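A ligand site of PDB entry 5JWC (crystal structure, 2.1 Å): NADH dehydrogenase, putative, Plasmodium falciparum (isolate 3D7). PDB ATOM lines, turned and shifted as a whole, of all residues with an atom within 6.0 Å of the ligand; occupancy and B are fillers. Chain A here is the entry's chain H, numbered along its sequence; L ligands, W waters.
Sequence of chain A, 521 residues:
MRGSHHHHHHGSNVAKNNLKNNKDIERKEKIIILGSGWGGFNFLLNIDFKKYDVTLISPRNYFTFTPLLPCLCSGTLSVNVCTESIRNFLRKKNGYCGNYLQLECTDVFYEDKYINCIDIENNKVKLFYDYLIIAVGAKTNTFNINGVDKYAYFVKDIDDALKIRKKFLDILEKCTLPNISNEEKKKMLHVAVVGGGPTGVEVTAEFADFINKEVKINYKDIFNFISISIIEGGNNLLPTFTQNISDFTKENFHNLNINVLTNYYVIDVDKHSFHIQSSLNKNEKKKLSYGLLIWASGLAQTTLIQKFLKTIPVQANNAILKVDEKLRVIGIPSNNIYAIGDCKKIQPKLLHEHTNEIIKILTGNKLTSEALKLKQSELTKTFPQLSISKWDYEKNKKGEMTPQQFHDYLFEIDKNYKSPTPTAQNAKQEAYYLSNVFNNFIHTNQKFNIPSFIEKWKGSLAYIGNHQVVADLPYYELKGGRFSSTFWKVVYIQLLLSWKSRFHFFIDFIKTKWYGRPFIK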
ATOM      1  N   CYS A  71       1.117   5.400  -9.653  1.00  0.00           N
ATOM      2  CA  CYS A  71       0.255   4.569 -10.529  1.00  0.00           C
ATOM      3  C   CYS A  71       0.806   4.457 -11.941  1.00  0.00           C
ATOM      4  O   CYS A  71       0.557   3.495 -12.642  1.00  0.00           O
ATOM      5  CB  CYS A  71      -1.143   5.158 -10.587  1.00  0.00           C
ATOM      6  SG  CYS A  71      -2.042   5.049  -9.059  1.00  0.00           S
ATOM      7  N   THR A  76      -0.917   1.268 -13.829  1.00  0.00           N
ATOM      8  CA  THR A  76      -2.284   1.260 -13.307  1.00  0.00           C
ATOM      9  C   THR A  76      -3.121   2.424 -13.881  1.00  0.00           C
ATOM     10  O   THR A  76      -4.318   2.275 -14.134  1.00  0.00           O
ATOM     11  CB  THR A  76      -2.280   1.326 -11.746  1.00  0.00           C
ATOM     12  OG1 THR A  76      -1.813   0.073 -11.235  1.00  0.00           O
ATOM     13  CG2 THR A  76      -3.667   1.585 -11.200  1.00  0.00           C
ATOM     14  N   GLU A 206       2.546  -0.583  -5.782  1.00  0.00           N
ATOM     15  CA  GLU A 206       2.150  -0.699  -7.187  1.00  0.00           C
ATOM     16  C   GLU A 206       2.971  -1.740  -7.921  1.00  0.00           C
ATOM     17  O   GLU A 206       2.429  -2.523  -8.696  1.00  0.00           O
ATOM     18  CB  GLU A 206       2.268   0.663  -7.867  1.00  0.00           C
ATOM     19  CG  GLU A 206       1.102   1.584  -7.561  1.00  0.00           C
ATOM     20  CD  GLU A 206      -0.195   1.094  -8.193  1.00  0.00           C
ATOM     21  OE1 GLU A 206      -1.283   1.475  -7.710  1.00  0.00           O
ATOM     22  OE2 GLU A 206      -0.142   0.329  -9.178  1.00  0.00           O
ATOM     23  N   ALA A 208       4.406  -4.286  -6.409  1.00  0.00           N
ATOM     24  CA  ALA A 208       4.039  -5.575  -5.845  1.00  0.00           C
ATOM     25  C   ALA A 208       2.778  -6.123  -6.511  1.00  0.00           C
ATOM     26  O   ALA A 208       2.723  -7.313  -6.818  1.00  0.00           O
ATOM     27  CB  ALA A 208       3.852  -5.489  -4.320  1.00  0.00           C
ATOM     28  N   ASP A 209       1.785  -5.265  -6.743  1.00  0.00           N
ATOM     29  CA  ASP A 209       0.559  -5.673  -7.434  1.00  0.00           C
ATOM     30  C   ASP A 209       0.845  -6.116  -8.876  1.00  0.00           C
ATOM     31  O   ASP A 209       0.397  -7.179  -9.321  1.00  0.00           O
ATOM     32  CB  ASP A 209      -0.457  -4.547  -7.491  1.00  0.00           C
ATOM     33  CG  ASP A 209      -1.067  -4.227  -6.119  1.00  0.00           C
ATOM     34  OD1 ASP A 209      -0.862  -4.980  -5.139  1.00  0.00           O
ATOM     35  OD2 ASP A 209      -1.786  -3.204  -6.046  1.00  0.00           O
ATOM     36  N   PHE A 210       1.585  -5.280  -9.594  1.00  0.00           N
ATOM     37  CA  PHE A 210       1.988  -5.592 -10.971  1.00  0.00           C
ATOM     38  C   PHE A 210       2.716  -6.953 -11.016  1.00  0.00           C
ATOM     39  O   PHE A 210       2.335  -7.844 -11.789  1.00  0.00           O
ATOM     40  CB  PHE A 210       2.886  -4.462 -11.494  1.00  0.00           C
ATOM     41  CG  PHE A 210       3.155  -4.514 -12.968  1.00  0.00           C
ATOM     42  CD1 PHE A 210       2.299  -5.180 -13.825  1.00  0.00           C
ATOM     43  CD2 PHE A 210       4.254  -3.877 -13.500  1.00  0.00           C
ATOM     44  CE1 PHE A 210       2.548  -5.219 -15.185  1.00  0.00           C
ATOM     45  CE2 PHE A 210       4.513  -3.921 -14.875  1.00  0.00           C
ATOM     46  CZ  PHE A 210       3.641  -4.597 -15.710  1.00  0.00           C
ATOM     47  N   ASN A 212       2.682  -9.386  -8.810  1.00  0.00           N
ATOM     48  CA  ASN A 212       1.781 -10.461  -8.418  1.00  0.00           C
ATOM     49  C   ASN A 212       0.669 -10.774  -9.406  1.00  0.00           C
ATOM     50  O   ASN A 212       0.066 -11.834  -9.325  1.00  0.00           O
ATOM     51  CB  ASN A 212       1.151 -10.157  -7.069  1.00  0.00           C
ATOM     52  CG  ASN A 212       2.051 -10.561  -5.923  1.00  0.00           C
ATOM     53  OD1 ASN A 212       2.772 -11.545  -6.016  1.00  0.00           O
ATOM     54  ND2 ASN A 212       2.036  -9.780  -4.843  1.00  0.00           N
ATOM     55  N   LYS A 213       0.372  -9.850 -10.327  1.00  0.00           N
ATOM     56  CA  LYS A 213      -0.704 -10.101 -11.270  1.00  0.00           C
ATOM     57  C   LYS A 213      -0.201 -10.316 -12.707  1.00  0.00           C
ATOM     58  O   LYS A 213       0.031 -11.449 -13.107  1.00  0.00           O
ATOM     59  CB  LYS A 213      -1.713  -8.962 -11.239  1.00  0.00           C
ATOM     60  CG  LYS A 213      -3.016  -9.292 -11.967  1.00  0.00           C
ATOM     61  CD  LYS A 213      -3.985  -8.140 -11.927  1.00  0.00           C
ATOM     62  CE  LYS A 213      -5.391  -8.559 -12.337  1.00  0.00           C
ATOM     63  NZ  LYS A 213      -6.323  -7.394 -12.226  1.00  0.00           N
ATOM     64  N   GLU A 214      -0.025  -9.239 -13.467  1.00  0.00           N
ATOM     65  CA  GLU A 214       0.325  -9.367 -14.873  1.00  0.00           C
ATOM     66  C   GLU A 214       1.687 -10.000 -15.109  1.00  0.00           C
ATOM     67  O   GLU A 214       1.860 -10.771 -16.032  1.00  0.00           O
ATOM     68  CB  GLU A 214       0.258  -8.010 -15.577  1.00  0.00           C
ATOM     69  CG  GLU A 214      -1.171  -7.466 -15.698  1.00  0.00           C
ATOM     70  CD  GLU A 214      -1.605  -6.646 -14.482  1.00  0.00           C
ATOM     71  OE1 GLU A 214      -0.854  -6.599 -13.466  1.00  0.00           O
ATOM     72  OE2 GLU A 214      -2.697  -6.052 -14.537  1.00  0.00           O
ATOM     73  N   LEU A 256       2.852  -9.418   1.756  1.00  0.00           N
ATOM     74  CA  LEU A 256       3.118  -9.429   0.317  1.00  0.00           C
ATOM     75  C   LEU A 256       4.560  -9.865   0.002  1.00  0.00           C
ATOM     76  O   LEU A 256       4.976  -9.846  -1.156  1.00  0.00           O
ATOM     77  CB  LEU A 256       2.843  -8.045  -0.291  1.00  0.00           C
ATOM     78  CG  LEU A 256       1.364  -7.663  -0.455  1.00  0.00           C
ATOM     79  CD1 LEU A 256       1.203  -6.172  -0.804  1.00  0.00           C
ATOM     80  CD2 LEU A 256       0.682  -8.534  -1.523  1.00  0.00           C
ATOM     81  N   TYR A 463      -2.223   4.370  -1.074  1.00  0.00           N
ATOM     82  CA  TYR A 463      -2.467   3.006  -1.500  1.00  0.00           C
ATOM     83  C   TYR A 463      -1.311   2.093  -1.080  1.00  0.00           C
ATOM     84  O   TYR A 463      -0.160   2.391  -1.378  1.00  0.00           O
ATOM     85  CB  TYR A 463      -2.659   2.934  -3.021  1.00  0.00           C
ATOM     86  CG  TYR A 463      -2.906   1.506  -3.478  1.00  0.00           C
ATOM     87  CD1 TYR A 463      -4.095   0.875  -3.184  1.00  0.00           C
ATOM     88  CD2 TYR A 463      -1.929   0.794  -4.154  1.00  0.00           C
ATOM     89  CE1 TYR A 463      -4.333  -0.437  -3.573  1.00  0.00           C
ATOM     90  CE2 TYR A 463      -2.143  -0.537  -4.542  1.00  0.00           C
ATOM     91  CZ  TYR A 463      -3.358  -1.137  -4.255  1.00  0.00           C
ATOM     92  OH  TYR A 463      -3.605  -2.444  -4.630  1.00  0.00           O
ATOM     93  N   GLY A 465      -1.142  -1.540  -1.404  1.00  0.00           N
ATOM     94  CA  GLY A 465      -1.012  -2.839  -2.041  1.00  0.00           C
ATOM     95  C   GLY A 465      -2.173  -3.779  -1.765  1.00  0.00           C
ATOM     96  O   GLY A 465      -2.845  -3.692  -0.734  1.00  0.00           O
ATOM     97  N   ASN A 466      -2.419  -4.679  -2.713  1.00  0.00           N
ATOM     98  CA  ASN A 466      -3.438  -5.721  -2.588  1.00  0.00           C
ATOM     99  C   ASN A 466      -4.795  -5.172  -2.167  1.00  0.00           C
ATOM    100  O   ASN A 466      -5.420  -5.692  -1.240  1.00  0.00           O
ATOM    101  CB  ASN A 466      -2.985  -6.793  -1.581  1.00  0.00           C
ATOM    102  CG  ASN A 466      -3.858  -8.056  -1.658  1.00  0.00           C
ATOM    103  OD1 ASN A 466      -4.303  -8.450  -2.729  1.00  0.00           O
ATOM    104  ND2 ASN A 466      -4.104  -8.679  -0.508  1.00  0.00           N
ATOM    105  N   HIS A 467      -5.222  -4.107  -2.862  1.00  0.00           N
ATOM    106  CA  HIS A 467      -6.530  -3.468  -2.685  1.00  0.00           C
ATOM    107  C   HIS A 467      -6.652  -2.607  -1.445  1.00  0.00           C
ATOM    108  O   HIS A 467      -7.687  -1.982  -1.223  1.00  0.00           O
ATOM    109  CB  HIS A 467      -7.651  -4.519  -2.664  1.00  0.00           C
ATOM    110  CG  HIS A 467      -7.701  -5.377  -3.885  1.00  0.00           C
ATOM    111  ND1 HIS A 467      -6.839  -6.430  -4.098  1.00  0.00           N
ATOM    112  CD2 HIS A 467      -8.521  -5.348  -4.961  1.00  0.00           C
ATOM    113  CE1 HIS A 467      -7.119  -7.012  -5.246  1.00  0.00           C
ATOM    114  NE2 HIS A 467      -8.134  -6.367  -5.797  1.00  0.00           N
ATOM    115  N   VAL A 469      -6.221   0.491   0.958  1.00  0.00           N
ATOM    116  CA  VAL A 469      -5.985   1.923   1.056  1.00  0.00           C
ATOM    117  C   VAL A 469      -6.051   2.344   2.518  1.00  0.00           C
ATOM    118  O   VAL A 469      -6.945   1.906   3.260  1.00  0.00           O
ATOM    119  CB  VAL A 469      -7.006   2.725   0.227  1.00  0.00           C
ATOM    120  CG1 VAL A 469      -7.008   4.203   0.634  1.00  0.00           C
ATOM    121  CG2 VAL A 469      -6.727   2.574  -1.292  1.00  0.00           C
ATOM    122  N   SER A 485     -10.543   0.956  -1.311  1.00  0.00           N
ATOM    123  CA  SER A 485     -10.146   1.319  -2.675  1.00  0.00           C
ATOM    124  C   SER A 485     -11.255   2.157  -3.329  1.00  0.00           C
ATOM    125  O   SER A 485     -10.960   3.010  -4.168  1.00  0.00           O
ATOM    126  CB  SER A 485      -9.819   0.088  -3.535  1.00  0.00           C
ATOM    127  OG  SER A 485     -10.988  -0.652  -3.853  1.00  0.00           O
ATOM    128  N   THR A 486     -12.510   1.925  -2.950  1.00  0.00           N
ATOM    129  CA  THR A 486     -13.608   2.716  -3.493  1.00  0.00           C
ATOM    130  C   THR A 486     -13.530   4.143  -2.998  1.00  0.00           C
ATOM    131  O   THR A 486     -13.780   5.102  -3.724  1.00  0.00           O
ATOM    132  CB  THR A 486     -14.998   2.120  -3.122  1.00  0.00           C
ATOM    133  OG1 THR A 486     -15.055   0.751  -3.528  1.00  0.00           O
ATOM    134  CG2 THR A 486     -16.092   2.878  -3.847  1.00  0.00           C
ATOM    135  N   TRP A 488     -10.831   5.760  -2.134  1.00  0.00           N
ATOM    136  CA  TRP A 488      -9.707   6.383  -2.835  1.00  0.00           C
ATOM    137  C   TRP A 488     -10.178   6.944  -4.193  1.00  0.00           C
ATOM    138  O   TRP A 488      -9.895   8.094  -4.532  1.00  0.00           O
ATOM    139  CB  TRP A 488      -8.616   5.331  -3.000  1.00  0.00           C
ATOM    140  CG  TRP A 488      -7.327   5.759  -3.599  1.00  0.00           C
ATOM    141  CD1 TRP A 488      -6.179   6.067  -2.926  1.00  0.00           C
ATOM    142  CD2 TRP A 488      -7.013   5.865  -4.988  1.00  0.00           C
ATOM    143  NE1 TRP A 488      -5.177   6.367  -3.816  1.00  0.00           N
ATOM    144  CE2 TRP A 488      -5.662   6.252  -5.100  1.00  0.00           C
ATOM    145  CE3 TRP A 488      -7.759   5.673  -6.168  1.00  0.00           C
ATOM    146  CZ2 TRP A 488      -5.039   6.456  -6.318  1.00  0.00           C
ATOM    147  CZ3 TRP A 488      -7.125   5.869  -7.391  1.00  0.00           C
ATOM    148  CH2 TRP A 488      -5.779   6.261  -7.457  1.00  0.00           C
ATOM    149  N   LYS A 489     -10.928   6.147  -4.939  1.00  0.00           N
ATOM    150  CA  LYS A 489     -11.433   6.565  -6.262  1.00  0.00           C
ATOM    151  C   LYS A 489     -12.400   7.749  -6.160  1.00  0.00           C
ATOM    152  O   LYS A 489     -12.318   8.695  -6.945  1.00  0.00           O
ATOM    153  CB  LYS A 489     -12.115   5.387  -6.960  1.00  0.00           C
ATOM    154  CG  LYS A 489     -11.175   4.218  -7.276  1.00  0.00           C
ATOM    155  CD  LYS A 489     -11.901   3.195  -8.129  1.00  0.00           C
ATOM    156  CE  LYS A 489     -11.008   2.028  -8.500  1.00  0.00           C
ATOM    157  NZ  LYS A 489     -10.726   1.187  -7.327  1.00  0.00           N
ATOM    158  N   PHE A 509      -9.442   2.519 -15.170  1.00  0.00           N
ATOM    159  CA  PHE A 509      -9.773   1.442 -14.247  1.00  0.00           C
ATOM    160  C   PHE A 509     -10.570   0.345 -14.943  1.00  0.00           C
ATOM    161  O   PHE A 509     -10.326  -0.841 -14.681  1.00  0.00           O
ATOM    162  CB  PHE A 509     -10.498   1.990 -13.028  1.00  0.00           C
ATOM    163  CG  PHE A 509      -9.529   2.524 -11.988  1.00  0.00           C
ATOM    164  CD1 PHE A 509      -8.607   1.662 -11.396  1.00  0.00           C
ATOM    165  CD2 PHE A 509      -9.514   3.864 -11.638  1.00  0.00           C
ATOM    166  CE1 PHE A 509      -7.711   2.130 -10.471  1.00  0.00           C
ATOM    167  CE2 PHE A 509      -8.628   4.330 -10.712  1.00  0.00           C
ATOM    168  CZ  PHE A 509      -7.715   3.457 -10.122  1.00  0.00           C
ATOM    169  N   THR A 512      -7.913  -1.583 -17.028  1.00  0.00           N
ATOM    170  CA  THR A 512      -7.043  -2.394 -16.199  1.00  0.00           C
ATOM    171  C   THR A 512      -7.780  -3.625 -15.661  1.00  0.00           C
ATOM    172  O   THR A 512      -7.220  -4.716 -15.623  1.00  0.00           O
ATOM    173  CB  THR A 512      -6.473  -1.538 -15.064  1.00  0.00           C
ATOM    174  OG1 THR A 512      -5.514  -0.629 -15.636  1.00  0.00           O
ATOM    175  CG2 THR A 512      -5.760  -2.372 -14.035  1.00  0.00           C
ATOM    176  N   ARG A 517      -2.818  -4.447 -16.960  1.00  0.00           N
ATOM    177  CA  ARG A 517      -1.834  -3.414 -17.229  1.00  0.00           C
ATOM    178  C   ARG A 517      -1.037  -3.691 -18.502  1.00  0.00           C
ATOM    179  O   ARG A 517      -0.740  -4.840 -18.800  1.00  0.00           O
ATOM    180  CB  ARG A 517      -0.869  -3.314 -16.040  1.00  0.00           C
ATOM    181  CG  ARG A 517      -1.512  -2.782 -14.744  1.00  0.00           C
ATOM    182  CD  ARG A 517      -0.523  -2.988 -13.614  1.00  0.00           C
ATOM    183  NE  ARG A 517      -1.037  -2.515 -12.347  1.00  0.00           N
ATOM    184  CZ  ARG A 517      -1.624  -3.272 -11.428  1.00  0.00           C
ATOM    185  NH1 ARG A 517      -1.754  -4.599 -11.606  1.00  0.00           N
ATOM    186  NH2 ARG A 517      -2.049  -2.703 -10.316  1.00  0.00           N
HETATM  187  C1  LIG L   1      -4.513   2.501  -6.751  1.00  0.00           C
HETATM  188  C2  LIG L   1      -4.155   1.196  -7.098  1.00  0.00           C
HETATM  189  C3  LIG L   1      -5.121   0.167  -7.117  1.00  0.00           C
HETATM  190  C4  LIG L   1      -6.455   0.451  -6.784  1.00  0.00           C
HETATM  191  C5  LIG L   1      -6.814   1.765  -6.433  1.00  0.00           C
HETATM  192  C6  LIG L   1      -5.859   2.796  -6.423  1.00  0.00           C
HETATM  193  O1  LIG L   1      -2.415 -11.502  -4.854  1.00  0.00           O
HETATM  194  C7  LIG L   1      -7.488  -0.669  -6.809  1.00  0.00           C
HETATM  195  C8  LIG L   1      -7.093  -2.022  -7.157  1.00  0.00           C
HETATM  196  C9  LIG L   1      -5.683  -2.287  -7.518  1.00  0.00           C
HETATM  197  C10 LIG L   1      -5.093  -3.640  -7.856  1.00  0.00           C
HETATM  198  C11 LIG L   1      -5.115  -4.633  -6.883  1.00  0.00           C
HETATM  199  C12 LIG L   1      -4.543  -5.871  -7.128  1.00  0.00           C
HETATM  200  C13 LIG L   1      -3.910  -6.095  -8.335  1.00  0.00           C
HETATM  201  C14 LIG L   1      -3.843  -5.099  -9.272  1.00  0.00           C
HETATM  202  C15 LIG L   1      -4.426  -3.869  -9.038  1.00  0.00           C
HETATM  203  O2  LIG L   1      -8.645  -0.442  -6.524  1.00  0.00           O
HETATM  204  N1  LIG L   1      -4.724  -1.211  -7.484  1.00  0.00           N
HETATM  205  C16 LIG L   1      -3.231  -7.386  -8.699  1.00  0.00           C
HETATM  206  C17 LIG L   1      -3.000  -8.430  -7.636  1.00  0.00           C
HETATM  207  C18 LIG L   1      -2.507  -8.129  -6.368  1.00  0.00           C
HETATM  208  C19 LIG L   1      -2.315  -9.153  -5.440  1.00  0.00           C
HETATM  209  C20 LIG L   1      -2.590 -10.468  -5.803  1.00  0.00           C
HETATM  210  C21 LIG L   1      -3.072 -10.777  -7.075  1.00  0.00           C
HETATM  211  C22 LIG L   1      -3.270  -9.761  -7.983  1.00  0.00           C
HETATM  212  C23 LIG L   1      -8.128  -3.123  -7.176  1.00  0.00           C
HETATM  213  F1  LIG L   1      -8.067   2.043  -6.115  1.00  0.00           F
HETATM  214  C24 LIG L   1      -3.582 -11.939  -4.183  1.00  0.00           C
HETATM  215  F2  LIG L   1      -3.577 -11.470  -2.930  1.00  0.00           F
HETATM  216  F3  LIG L   1      -3.595 -13.277  -4.161  1.00  0.00           F
HETATM  217  F4  LIG L   1      -4.692 -11.514  -4.809  1.00  0.00           F
HETATM  218  O   HOH W   1      -2.260  -1.457  -8.141  1.00  0.00           O
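Water W1 lies within hydrogen-bond range of NH2 of Arg 517 (2.5 Å), N1 of the ligand (2.6 Å), OD2 of Asp 209 (2.8 Å), OE2 of Glu 206 (3.0 Å) and OG1 of Thr 76 (3.5 Å).
OD1 of Asn 466 sits close to F2 of the ligand, 3.1 Å away. OE1 of Glu 206 touches C2 of the ligand, at 2.9 Å. Asp 209 touches the ligand (O to C16, 3.7 Å). Asn 212 touches the ligand. Lys 213 touches the ligand. His 467 touches the ligand. CB of Ser 485 touches O2 of the ligand (3.3 Å). Trp 488 touches the ligand. Arg 517 touches the ligand (NH2 to C15, 2.9 Å). Hydrophobic or aromatic side chains that line the ligand: Tyr 463, His 467 and Trp 488. 11 residues have an atom within 4 Å of the ligand: Glu 206, Asp 209, Asn 212, Lys 213, Tyr 463, Asn 466, His 467, Ser 485, Trp 488, Lys 489 and Arg 517. Along chain A the residues within 4 Å of the ligand span positions 206 to 517.
The side-chain amino group (NZ) of Lys 489 lies within hydrogen-bond range of an oxygen (O2) of the ligand, 2.8 Å away. The side-chain hydroxyl (OH) of Tyr 463 lies within hydrogen-bond range of a nitrogen (N1) of the ligand (3.3 Å).
OD1 of Asp 209 is in hydrogen-bond range of N of Asn 466 (2.9 Å). The side-chain hydroxyl (OH) of Tyr 463 sits at hydrogen-bond distance from the backbone NH (N) of Asn 466 (3.2 Å). NH1 of Arg 517 lies within salt-bridge range of OE1 of Glu 214, at 2.9 Å. The guanidinium group (NE) of Arg 517 sits at hydrogen-bond distance from the side-chain hydroxyl (OG1) of Thr 76 (2.9 Å). The guanidinium group (NH2) of Arg 517 is in salt-bridge range of the side-chain carboxylate (OE2) of Glu 206 (3.8 Å). ND2 of Asn 212 is in hydrogen-bond range of O of Ala 208 (3.2 Å). The side-chain hydroxyl (OG1) of Thr 76 is in hydrogen-bond range of the side-chain carboxylate (OE2) of Glu 206. The side-chain hydroxyl of Tyr 463 lies within hydrogen-bond range of the side-chain carboxylate of Asp 209 (2.4 Å).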
